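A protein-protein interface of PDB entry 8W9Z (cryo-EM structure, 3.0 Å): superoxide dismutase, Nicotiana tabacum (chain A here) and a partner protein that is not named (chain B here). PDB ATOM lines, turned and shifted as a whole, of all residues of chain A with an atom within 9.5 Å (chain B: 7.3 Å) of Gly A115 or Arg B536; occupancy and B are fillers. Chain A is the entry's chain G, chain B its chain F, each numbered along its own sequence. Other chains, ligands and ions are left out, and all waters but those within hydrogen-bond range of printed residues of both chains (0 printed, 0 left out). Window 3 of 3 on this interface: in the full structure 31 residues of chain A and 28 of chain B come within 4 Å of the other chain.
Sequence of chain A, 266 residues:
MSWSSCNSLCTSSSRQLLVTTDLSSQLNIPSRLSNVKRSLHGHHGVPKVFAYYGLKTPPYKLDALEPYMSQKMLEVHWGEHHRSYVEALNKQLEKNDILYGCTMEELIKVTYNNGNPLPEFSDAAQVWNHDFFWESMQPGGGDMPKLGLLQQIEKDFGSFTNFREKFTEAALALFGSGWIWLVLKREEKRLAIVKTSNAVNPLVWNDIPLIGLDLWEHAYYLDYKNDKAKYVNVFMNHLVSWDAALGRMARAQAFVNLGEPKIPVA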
ATOM      1  N   ILE A 108      -0.360  26.389  -6.950  1.00  0.00           N
ATOM      2  CA  ILE A 108      -1.788  26.683  -6.850  1.00  0.00           C
ATOM      3  C   ILE A 108      -2.433  26.669  -8.231  1.00  0.00           C
ATOM      4  O   ILE A 108      -3.502  26.078  -8.433  1.00  0.00           O
ATOM      5  CB  ILE A 108      -2.008  28.028  -6.135  1.00  0.00           C
ATOM      6  CG1 ILE A 108      -1.510  27.944  -4.693  1.00  0.00           C
ATOM      7  CG2 ILE A 108      -3.475  28.414  -6.167  1.00  0.00           C
ATOM      8  CD1 ILE A 108      -1.536  29.261  -3.965  1.00  0.00           C
ATOM      9  N   LYS A 109      -1.782  27.302  -9.207  1.00  0.00           N
ATOM     10  CA  LYS A 109      -2.345  27.360 -10.552  1.00  0.00           C
ATOM     11  C   LYS A 109      -2.337  25.991 -11.222  1.00  0.00           C
ATOM     12  O   LYS A 109      -3.261  25.660 -11.975  1.00  0.00           O
ATOM     13  CB  LYS A 109      -1.579  28.374 -11.400  1.00  0.00           C
ATOM     14  CG  LYS A 109      -1.665  29.801 -10.892  1.00  0.00           C
ATOM     15  CD  LYS A 109      -0.934  30.757 -11.818  1.00  0.00           C
ATOM     16  CE  LYS A 109      -1.497  30.691 -13.228  1.00  0.00           C
ATOM     17  NZ  LYS A 109      -2.942  31.048 -13.266  1.00  0.00           N
ATOM     18  N   VAL A 110      -1.308  25.179 -10.968  1.00  0.00           N
ATOM     19  CA  VAL A 110      -1.241  23.867 -11.600  1.00  0.00           C
ATOM     20  C   VAL A 110      -2.171  22.863 -10.930  1.00  0.00           C
ATOM     21  O   VAL A 110      -2.566  21.878 -11.566  1.00  0.00           O
ATOM     22  CB  VAL A 110       0.206  23.343 -11.617  1.00  0.00           C
ATOM     23  CG1 VAL A 110       0.601  22.780 -10.262  1.00  0.00           C
ATOM     24  CG2 VAL A 110       0.388  22.301 -12.712  1.00  0.00           C
ATOM     25  N   THR A 111      -2.542  23.085  -9.669  1.00  0.00           N
ATOM     26  CA  THR A 111      -3.514  22.228  -9.006  1.00  0.00           C
ATOM     27  C   THR A 111      -4.948  22.699  -9.202  1.00  0.00           C
ATOM     28  O   THR A 111      -5.876  21.910  -8.995  1.00  0.00           O
ATOM     29  CB  THR A 111      -3.212  22.136  -7.509  1.00  0.00           C
ATOM     30  OG1 THR A 111      -3.102  23.454  -6.957  1.00  0.00           O
ATOM     31  CG2 THR A 111      -1.915  21.381  -7.274  1.00  0.00           C
ATOM     32  N   TYR A 112      -5.152  23.960  -9.587  1.00  0.00           N
ATOM     33  CA  TYR A 112      -6.497  24.414  -9.924  1.00  0.00           C
ATOM     34  C   TYR A 112      -7.005  23.728 -11.186  1.00  0.00           C
ATOM     35  O   TYR A 112      -8.185  23.370 -11.273  1.00  0.00           O
ATOM     36  CB  TYR A 112      -6.511  25.933 -10.087  1.00  0.00           C
ATOM     37  CG  TYR A 112      -7.875  26.516 -10.367  1.00  0.00           C
ATOM     38  CD1 TYR A 112      -8.832  26.603  -9.369  1.00  0.00           C
ATOM     39  CD2 TYR A 112      -8.200  26.995 -11.627  1.00  0.00           C
ATOM     40  CE1 TYR A 112     -10.079  27.141  -9.618  1.00  0.00           C
ATOM     41  CE2 TYR A 112      -9.445  27.535 -11.888  1.00  0.00           C
ATOM     42  CZ  TYR A 112     -10.379  27.605 -10.879  1.00  0.00           C
ATOM     43  OH  TYR A 112     -11.619  28.142 -11.134  1.00  0.00           O
ATOM     44  N   ASN A 113      -6.125  23.540 -12.172  1.00  0.00           N
ATOM     45  CA  ASN A 113      -6.420  22.775 -13.386  1.00  0.00           C
ATOM     46  C   ASN A 113      -7.607  23.350 -14.156  1.00  0.00           C
ATOM     47  O   ASN A 113      -8.319  22.622 -14.853  1.00  0.00           O
ATOM     48  CB  ASN A 113      -6.651  21.295 -13.064  1.00  0.00           C
ATOM     49  CG  ASN A 113      -6.476  20.400 -14.273  1.00  0.00           C
ATOM     50  OD1 ASN A 113      -5.874  20.795 -15.270  1.00  0.00           O
ATOM     51  ND2 ASN A 113      -7.005  19.184 -14.190  1.00  0.00           N
ATOM     52  N   ASN A 114      -7.827  24.659 -14.030  1.00  0.00           N
ATOM     53  CA  ASN A 114      -8.820  25.388 -14.819  1.00  0.00           C
ATOM     54  C   ASN A 114     -10.226  24.815 -14.617  1.00  0.00           C
ATOM     55  O   ASN A 114     -10.884  24.355 -15.553  1.00  0.00           O
ATOM     56  CB  ASN A 114      -8.429  25.396 -16.302  1.00  0.00           C
ATOM     57  CG  ASN A 114      -9.259  26.364 -17.118  1.00  0.00           C
ATOM     58  OD1 ASN A 114      -9.848  27.300 -16.580  1.00  0.00           O
ATOM     59  ND2 ASN A 114      -9.310  26.142 -18.427  1.00  0.00           N
ATOM     60  N   GLY A 115     -10.677  24.847 -13.364  1.00  0.00           N
ATOM     61  CA  GLY A 115     -12.034  24.495 -13.016  1.00  0.00           C
ATOM     62  C   GLY A 115     -12.210  23.117 -12.411  1.00  0.00           C
ATOM     63  O   GLY A 115     -13.198  22.892 -11.704  1.00  0.00           O
ATOM     64  N   ASN A 116     -11.288  22.187 -12.672  1.00  0.00           N
ATOM     65  CA  ASN A 116     -11.355  20.822 -12.155  1.00  0.00           C
ATOM     66  C   ASN A 116     -10.174  20.618 -11.214  1.00  0.00           C
ATOM     67  O   ASN A 116      -9.141  20.055 -11.606  1.00  0.00           O
ATOM     68  CB  ASN A 116     -11.347  19.800 -13.292  1.00  0.00           C
ATOM     69  CG  ASN A 116     -11.533  18.379 -12.800  1.00  0.00           C
ATOM     70  OD1 ASN A 116     -10.563  17.664 -12.551  1.00  0.00           O
ATOM     71  ND2 ASN A 116     -12.786  17.961 -12.660  1.00  0.00           N
ATOM     72  N   PRO A 117     -10.293  21.054  -9.962  1.00  0.00           N
ATOM     73  CA  PRO A 117      -9.130  21.063  -9.069  1.00  0.00           C
ATOM     74  C   PRO A 117      -8.647  19.665  -8.719  1.00  0.00           C
ATOM     75  O   PRO A 117      -9.428  18.720  -8.590  1.00  0.00           O
ATOM     76  CB  PRO A 117      -9.646  21.793  -7.822  1.00  0.00           C
ATOM     77  CG  PRO A 117     -10.869  22.525  -8.275  1.00  0.00           C
ATOM     78  CD  PRO A 117     -11.474  21.660  -9.330  1.00  0.00           C
ATOM     79  N   LEU A 118      -7.330  19.549  -8.566  1.00  0.00           N
ATOM     80  CA  LEU A 118      -6.719  18.322  -8.094  1.00  0.00           C
ATOM     81  C   LEU A 118      -6.983  18.152  -6.598  1.00  0.00           C
ATOM     82  O   LEU A 118      -7.324  19.116  -5.908  1.00  0.00           O
ATOM     83  CB  LEU A 118      -5.219  18.343  -8.381  1.00  0.00           C
ATOM     84  CG  LEU A 118      -4.824  18.401  -9.858  1.00  0.00           C
ATOM     85  CD1 LEU A 118      -3.318  18.280 -10.018  1.00  0.00           C
ATOM     86  CD2 LEU A 118      -5.540  17.318 -10.647  1.00  0.00           C
ATOM     87  N   PHE A 121      -5.346  20.802  -4.242  1.00  0.00           N
ATOM     88  CA  PHE A 121      -5.461  22.238  -4.477  1.00  0.00           C
ATOM     89  C   PHE A 121      -5.973  22.961  -3.240  1.00  0.00           C
ATOM     90  O   PHE A 121      -5.437  24.007  -2.853  1.00  0.00           O
ATOM     91  CB  PHE A 121      -6.380  22.511  -5.665  1.00  0.00           C
ATOM     92  CG  PHE A 121      -6.850  23.935  -5.743  1.00  0.00           C
ATOM     93  CD1 PHE A 121      -6.004  24.933  -6.190  1.00  0.00           C
ATOM     94  CD2 PHE A 121      -8.138  24.276  -5.366  1.00  0.00           C
ATOM     95  CE1 PHE A 121      -6.432  26.244  -6.260  1.00  0.00           C
ATOM     96  CE2 PHE A 121      -8.571  25.583  -5.435  1.00  0.00           C
ATOM     97  CZ  PHE A 121      -7.718  26.569  -5.881  1.00  0.00           C
ATOM     98  N   SER A 197     -14.554  31.527  -3.288  1.00  0.00           N
ATOM     99  CA  SER A 197     -15.165  30.374  -2.647  1.00  0.00           C
ATOM    100  C   SER A 197     -14.331  29.957  -1.438  1.00  0.00           C
ATOM    101  O   SER A 197     -13.502  30.720  -0.934  1.00  0.00           O
ATOM    102  CB  SER A 197     -15.325  29.234  -3.651  1.00  0.00           C
ATOM    103  OG  SER A 197     -14.067  28.764  -4.096  1.00  0.00           O
ATOM    104  N   VAL A 200     -10.496  28.987  -2.953  1.00  0.00           N
ATOM    105  CA  VAL A 200      -9.964  29.588  -4.169  1.00  0.00           C
ATOM    106  C   VAL A 200      -9.407  30.969  -3.855  1.00  0.00           C
ATOM    107  O   VAL A 200     -10.045  31.775  -3.166  1.00  0.00           O
ATOM    108  CB  VAL A 200     -11.048  29.651  -5.255  1.00  0.00           C
ATOM    109  CG1 VAL A 200     -10.589  30.511  -6.420  1.00  0.00           C
ATOM    110  CG2 VAL A 200     -11.387  28.250  -5.738  1.00  0.00           C
ATOM    111  N   VAL A 204      -5.444  32.188  -9.236  1.00  0.00           N
ATOM    112  CA  VAL A 204      -5.874  31.351 -10.347  1.00  0.00           C
ATOM    113  C   VAL A 204      -6.239  32.177 -11.574  1.00  0.00           C
ATOM    114  O   VAL A 204      -6.331  31.628 -12.678  1.00  0.00           O
ATOM    115  CB  VAL A 204      -7.054  30.461  -9.916  1.00  0.00           C
ATOM    116  CG1 VAL A 204      -6.647  29.578  -8.750  1.00  0.00           C
ATOM    117  CG2 VAL A 204      -8.254  31.313  -9.545  1.00  0.00           C
ATOM    118  N   TRP A 205      -6.450  33.483 -11.414  1.00  0.00           N
ATOM    119  CA  TRP A 205      -6.773  34.365 -12.529  1.00  0.00           C
ATOM    120  C   TRP A 205      -5.655  35.350 -12.839  1.00  0.00           C
ATOM    121  O   TRP A 205      -5.883  36.317 -13.574  1.00  0.00           O
ATOM    122  CB  TRP A 205      -8.070  35.127 -12.250  1.00  0.00           C
ATOM    123  CG  TRP A 205      -9.245  34.247 -11.966  1.00  0.00           C
ATOM    124  CD1 TRP A 205      -9.889  33.431 -12.848  1.00  0.00           C
ATOM    125  CD2 TRP A 205      -9.928  34.106 -10.716  1.00  0.00           C
ATOM    126  NE1 TRP A 205     -10.926  32.783 -12.221  1.00  0.00           N
ATOM    127  CE2 TRP A 205     -10.971  33.181 -10.911  1.00  0.00           C
ATOM    128  CE3 TRP A 205      -9.755  34.669  -9.448  1.00  0.00           C
ATOM    129  CZ2 TRP A 205     -11.839  32.807  -9.889  1.00  0.00           C
ATOM    130  CZ3 TRP A 205     -10.618  34.296  -8.435  1.00  0.00           C
ATOM    131  CH2 TRP A 205     -11.646  33.375  -8.660  1.00  0.00           C
ATOM    132  N   ARG B 531     -26.152  16.461 -10.090  1.00  0.00           N
ATOM    133  CA  ARG B 531     -25.586  16.884  -8.815  1.00  0.00           C
ATOM    134  C   ARG B 531     -24.339  17.735  -9.006  1.00  0.00           C
ATOM    135  O   ARG B 531     -24.088  18.653  -8.212  1.00  0.00           O
ATOM    136  CB  ARG B 531     -25.251  15.668  -7.949  1.00  0.00           C
ATOM    137  CG  ARG B 531     -26.342  14.618  -7.888  1.00  0.00           C
ATOM    138  CD  ARG B 531     -26.075  13.629  -6.766  1.00  0.00           C
ATOM    139  NE  ARG B 531     -24.672  13.228  -6.712  1.00  0.00           N
ATOM    140  CZ  ARG B 531     -24.168  12.180  -7.351  1.00  0.00           C
ATOM    141  NH1 ARG B 531     -22.878  11.892  -7.242  1.00  0.00           N
ATOM    142  NH2 ARG B 531     -24.951  11.419  -8.102  1.00  0.00           N
ATOM    143  N   ASP B 532     -23.549  17.442 -10.041  1.00  0.00           N
ATOM    144  CA  ASP B 532     -22.329  18.201 -10.283  1.00  0.00           C
ATOM    145  C   ASP B 532     -22.640  19.651 -10.626  1.00  0.00           C
ATOM    146  O   ASP B 532     -21.975  20.568 -10.133  1.00  0.00           O
ATOM    147  CB  ASP B 532     -21.519  17.546 -11.402  1.00  0.00           C
ATOM    148  CG  ASP B 532     -20.097  18.065 -11.473  1.00  0.00           C
ATOM    149  OD1 ASP B 532     -19.675  18.776 -10.538  1.00  0.00           O
ATOM    150  OD2 ASP B 532     -19.402  17.759 -12.464  1.00  0.00           O
ATOM    151  N   ILE B 533     -23.649  19.878 -11.471  1.00  0.00           N
ATOM    152  CA  ILE B 533     -24.015  21.245 -11.834  1.00  0.00           C
ATOM    153  C   ILE B 533     -24.430  22.029 -10.597  1.00  0.00           C
ATOM    154  O   ILE B 533     -24.032  23.186 -10.412  1.00  0.00           O
ATOM    155  CB  ILE B 533     -25.124  21.240 -12.903  1.00  0.00           C
ATOM    156  CG1 ILE B 533     -24.606  20.627 -14.206  1.00  0.00           C
ATOM    157  CG2 ILE B 533     -25.638  22.649 -13.146  1.00  0.00           C
ATOM    158  CD1 ILE B 533     -25.626  20.619 -15.323  1.00  0.00           C
ATOM    159  N   SER B 534     -25.178  21.394  -9.733  1.00  0.00           N
ATOM    160  CA  SER B 534     -25.648  22.120  -8.591  1.00  0.00           C
ATOM    161  C   SER B 534     -24.497  22.570  -7.747  1.00  0.00           C
ATOM    162  O   SER B 534     -24.377  23.747  -7.442  1.00  0.00           O
ATOM    163  CB  SER B 534     -26.581  21.264  -7.768  1.00  0.00           C
ATOM    164  OG  SER B 534     -25.893  20.216  -7.121  1.00  0.00           O
ATOM    165  N   CYS B 535     -23.632  21.650  -7.362  1.00  0.00           N
ATOM    166  CA  CYS B 535     -22.570  22.025  -6.454  1.00  0.00           C
ATOM    167  C   CYS B 535     -21.616  23.039  -7.037  1.00  0.00           C
ATOM    168  O   CYS B 535     -21.214  23.971  -6.364  1.00  0.00           O
ATOM    169  CB  CYS B 535     -21.821  20.808  -5.957  1.00  0.00           C
ATOM    170  SG  CYS B 535     -20.988  19.858  -7.227  1.00  0.00           S
ATOM    171  N   ARG B 536     -21.264  22.880  -8.294  1.00  0.00           N
ATOM    172  CA  ARG B 536     -20.374  23.823  -8.888  1.00  0.00           C
ATOM    173  C   ARG B 536     -21.016  25.197  -8.884  1.00  0.00           C
ATOM    174  O   ARG B 536     -20.359  26.177  -8.589  1.00  0.00           O
ATOM    175  CB  ARG B 536     -20.009  23.413 -10.296  1.00  0.00           C
ATOM    176  CG  ARG B 536     -19.067  22.236 -10.370  1.00  0.00           C
ATOM    177  CD  ARG B 536     -18.909  21.786 -11.807  1.00  0.00           C
ATOM    178  NE  ARG B 536     -17.569  22.030 -12.315  1.00  0.00           N
ATOM    179  CZ  ARG B 536     -16.549  21.200 -12.147  1.00  0.00           C
ATOM    180  NH1 ARG B 536     -16.708  20.071 -11.473  1.00  0.00           N
ATOM    181  NH2 ARG B 536     -15.368  21.498 -12.653  1.00  0.00           N
ATOM    182  N   ARG B 537     -22.298  25.283  -9.188  1.00  0.00           N
ATOM    183  CA  ARG B 537     -22.967  26.564  -9.197  1.00  0.00           C
ATOM    184  C   ARG B 537     -22.970  27.166  -7.827  1.00  0.00           C
ATOM    185  O   ARG B 537     -22.799  28.362  -7.665  1.00  0.00           O
ATOM    186  CB  ARG B 537     -24.398  26.406  -9.650  1.00  0.00           C
ATOM    187  CG  ARG B 537     -24.578  26.318 -11.148  1.00  0.00           C
ATOM    188  CD  ARG B 537     -24.341  27.672 -11.779  1.00  0.00           C
ATOM    189  NE  ARG B 537     -25.063  28.715 -11.066  1.00  0.00           N
ATOM    190  CZ  ARG B 537     -25.107  29.982 -11.452  1.00  0.00           C
ATOM    191  NH1 ARG B 537     -24.476  30.361 -12.553  1.00  0.00           N
ATOM    192  NH2 ARG B 537     -25.785  30.869 -10.741  1.00  0.00           N
ATOM    193  N   ALA B 538     -23.207  26.342  -6.831  1.00  0.00           N
ATOM    194  CA  ALA B 538     -23.235  26.825  -5.472  1.00  0.00           C
ATOM    195  C   ALA B 538     -21.911  27.336  -4.987  1.00  0.00           C
ATOM    196  O   ALA B 538     -21.850  28.362  -4.331  1.00  0.00           O
ATOM    197  CB  ALA B 538     -23.696  25.720  -4.562  1.00  0.00           C
ATOM    198  N   LEU B 539     -20.838  26.628  -5.298  1.00  0.00           N
ATOM    199  CA  LEU B 539     -19.542  27.005  -4.783  1.00  0.00           C
ATOM    200  C   LEU B 539     -18.818  27.935  -5.713  1.00  0.00           C
ATOM    201  O   LEU B 539     -17.703  28.328  -5.443  1.00  0.00           O
ATOM    202  CB  LEU B 539     -18.706  25.774  -4.519  1.00  0.00           C
ATOM    203  CG  LEU B 539     -19.006  25.045  -3.223  1.00  0.00           C
ATOM    204  CD1 LEU B 539     -18.081  23.849  -3.085  1.00  0.00           C
ATOM    205  CD2 LEU B 539     -18.796  26.017  -2.079  1.00  0.00           C
ATOM    206  N   GLY B 540     -19.427  28.269  -6.833  1.00  0.00           N
ATOM    207  CA  GLY B 540     -18.826  29.221  -7.741  1.00  0.00           C
ATOM    208  C   GLY B 540     -17.756  28.657  -8.635  1.00  0.00           C
ATOM    209  O   GLY B 540     -16.703  29.255  -8.779  1.00  0.00           O
ATOM    210  N   LEU B 541     -18.021  27.519  -9.250  1.00  0.00           N
ATOM    211  CA  LEU B 541     -17.044  26.885 -10.118  1.00  0.00           C
ATOM    212  C   LEU B 541     -17.559  26.845 -11.553  1.00  0.00           C
ATOM    213  O   LEU B 541     -18.770  26.774 -11.781  1.00  0.00           O
ATOM    214  CB  LEU B 541     -16.721  25.460  -9.655  1.00  0.00           C
ATOM    215  CG  LEU B 541     -15.956  25.330  -8.336  1.00  0.00           C
ATOM    216  CD1 LEU B 541     -15.660  23.872  -8.028  1.00  0.00           C
ATOM    217  CD2 LEU B 541     -14.675  26.141  -8.379  1.00  0.00           C
ATOM    218  N   PRO B 542     -16.668  26.900 -12.544  1.00  0.00           N
ATOM    219  CA  PRO B 542     -17.120  26.936 -13.942  1.00  0.00           C
ATOM    220  C   PRO B 542     -17.805  25.636 -14.340  1.00  0.00           C
ATOM    221  O   PRO B 542     -17.298  24.544 -14.077  1.00  0.00           O
ATOM    222  CB  PRO B 542     -15.822  27.152 -14.731  1.00  0.00           C
ATOM    223  CG  PRO B 542     -14.860  27.725 -13.740  1.00  0.00           C
ATOM    224  CD  PRO B 542     -15.213  27.090 -12.431  1.00  0.00           C
ATOM    225  N   LEU B 543     -18.969  25.767 -14.980  1.00  0.00           N
ATOM    226  CA  LEU B 543     -19.677  24.598 -15.488  1.00  0.00           C
ATOM    227  C   LEU B 543     -19.103  24.123 -16.814  1.00  0.00           C
ATOM    228  O   LEU B 543     -19.105  22.918 -17.091  1.00  0.00           O
ATOM    229  CB  LEU B 543     -21.165  24.908 -15.648  1.00  0.00           C
ATOM    230  CG  LEU B 543     -21.939  25.288 -14.386  1.00  0.00           C
ATOM    231  CD1 LEU B 543     -23.384  25.608 -14.730  1.00  0.00           C
ATOM    232  CD2 LEU B 543     -21.864  24.173 -13.358  1.00  0.00           C
ATOM    233  N   GLU B 544     -18.614  25.044 -17.638  1.00  0.00           N
ATOM    234  CA  GLU B 544     -17.988  24.720 -18.908  1.00  0.00           C
ATOM    235  C   GLU B 544     -16.535  25.172 -18.877  1.00  0.00           C
ATOM    236  O   GLU B 544     -16.181  26.122 -18.173  1.00  0.00           O
ATOM    237  CB  GLU B 544     -18.728  25.382 -20.077  1.00  0.00           C
ATOM    238  CG  GLU B 544     -18.307  24.887 -21.451  1.00  0.00           C
ATOM    239  CD  GLU B 544     -18.665  23.432 -21.686  1.00  0.00           C
ATOM    240  OE1 GLU B 544     -19.622  22.940 -21.051  1.00  0.00           O
ATOM    241  OE2 GLU B 544     -17.989  22.778 -22.509  1.00  0.00           O
ATOM    242  N   GLU B 545     -15.696  24.476 -19.635  1.00  0.00           N
ATOM    243  CA  GLU B 545     -14.268  24.758 -19.660  1.00  0.00           C
ATOM    244  C   GLU B 545     -14.017  26.194 -20.104  1.00  0.00           C
ATOM    245  O   GLU B 545     -14.402  26.565 -21.224  1.00  0.00           O
ATOM    246  CB  GLU B 545     -13.552  23.785 -20.592  1.00  0.00           C
ATOM    247  CG  GLU B 545     -12.046  23.980 -20.657  1.00  0.00           C
ATOM    248  CD  GLU B 545     -11.362  22.948 -21.531  1.00  0.00           C
ATOM    249  OE1 GLU B 545     -12.063  22.062 -22.066  1.00  0.00           O
ATOM    250  OE2 GLU B 545     -10.126  23.022 -21.684  1.00  0.00           O
ATOM    251  N   PRO B 546     -13.396  27.030 -19.273  1.00  0.00           N
ATOM    252  CA  PRO B 546     -13.160  28.422 -19.671  1.00  0.00           C
ATOM    253  C   PRO B 546     -12.173  28.510 -20.824  1.00  0.00           C
ATOM    254  O   PRO B 546     -11.135  27.845 -20.833  1.00  0.00           O
ATOM    255  CB  PRO B 546     -12.590  29.064 -18.400  1.00  0.00           C
ATOM    256  CG  PRO B 546     -12.978  28.142 -17.287  1.00  0.00           C
ATOM    257  CD  PRO B 546     -12.976  26.773 -17.886  1.00  0.00           C
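O of Gly A115 sits at hydrogen-bond distance from NH2 of Arg B536 (2.7 Å).
The side-chain amide nitrogen (ND2) of Asn A114 lies within hydrogen-bond range of the backbone carbonyl oxygen (O) of Pro B546 (3.5 Å).
The side-chain carboxylate of Asp B532 is in salt-bridge range of the guanidinium group of Arg B536, 3.4 Å away.
O of Arg B536 is in hydrogen-bond range of N of Leu B541 (2.8 Å).
NE of Arg B536 is in hydrogen-bond range of O of Pro B542, at 3.1 Å.
Among the printed residues, pairs that only touch across the chains: Ser A197 with Leu B539 and Tyr A112 with Pro B542.
Gly A115 touches just one residue of chain B: Arg B536 (2.7 Å).
No residue of chain A comes within 4 Å of Cys B535.
Gly B540 touches none of the printed residues of chain A.
No residue of chain A comes within 4 Å of Leu B541.
Of chain A, only Tyr A112 (3.96 Å) comes within 4 Å of Pro B542.
Of the printed residues of chain B, Ser A197 touches Leu B539 (3.1 Å).
Of the printed residues of chain B, Tyr A112 touches Pro B542 (3.96 Å).
Of the printed residues of chain B, Asn A114 touches Pro B546 (3.3 Å).
Of the printed residues of chain A, Pro B546 touches Asn A114.
Of the printed residues of chain A, Leu B539 touches Ser A197.
The nearest residue of chain A that does not touch Arg B536 is Asn A116 (4.1 Å).
The nearest printed residue of chain A that does not touch Pro B546 is Gly A115 (5.4 Å).
Hydrophobic or aromatic side chains of chain A that line the printed part of chain B: Tyr A112.
Printed residues of chain B that touch a printed residue of chain A: Arg B536, Leu B539, Pro B542 and Pro B546.
Hydrophobic or aromatic side chains of chain B that line the printed part of chain A: Pro B542 and Pro B546.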
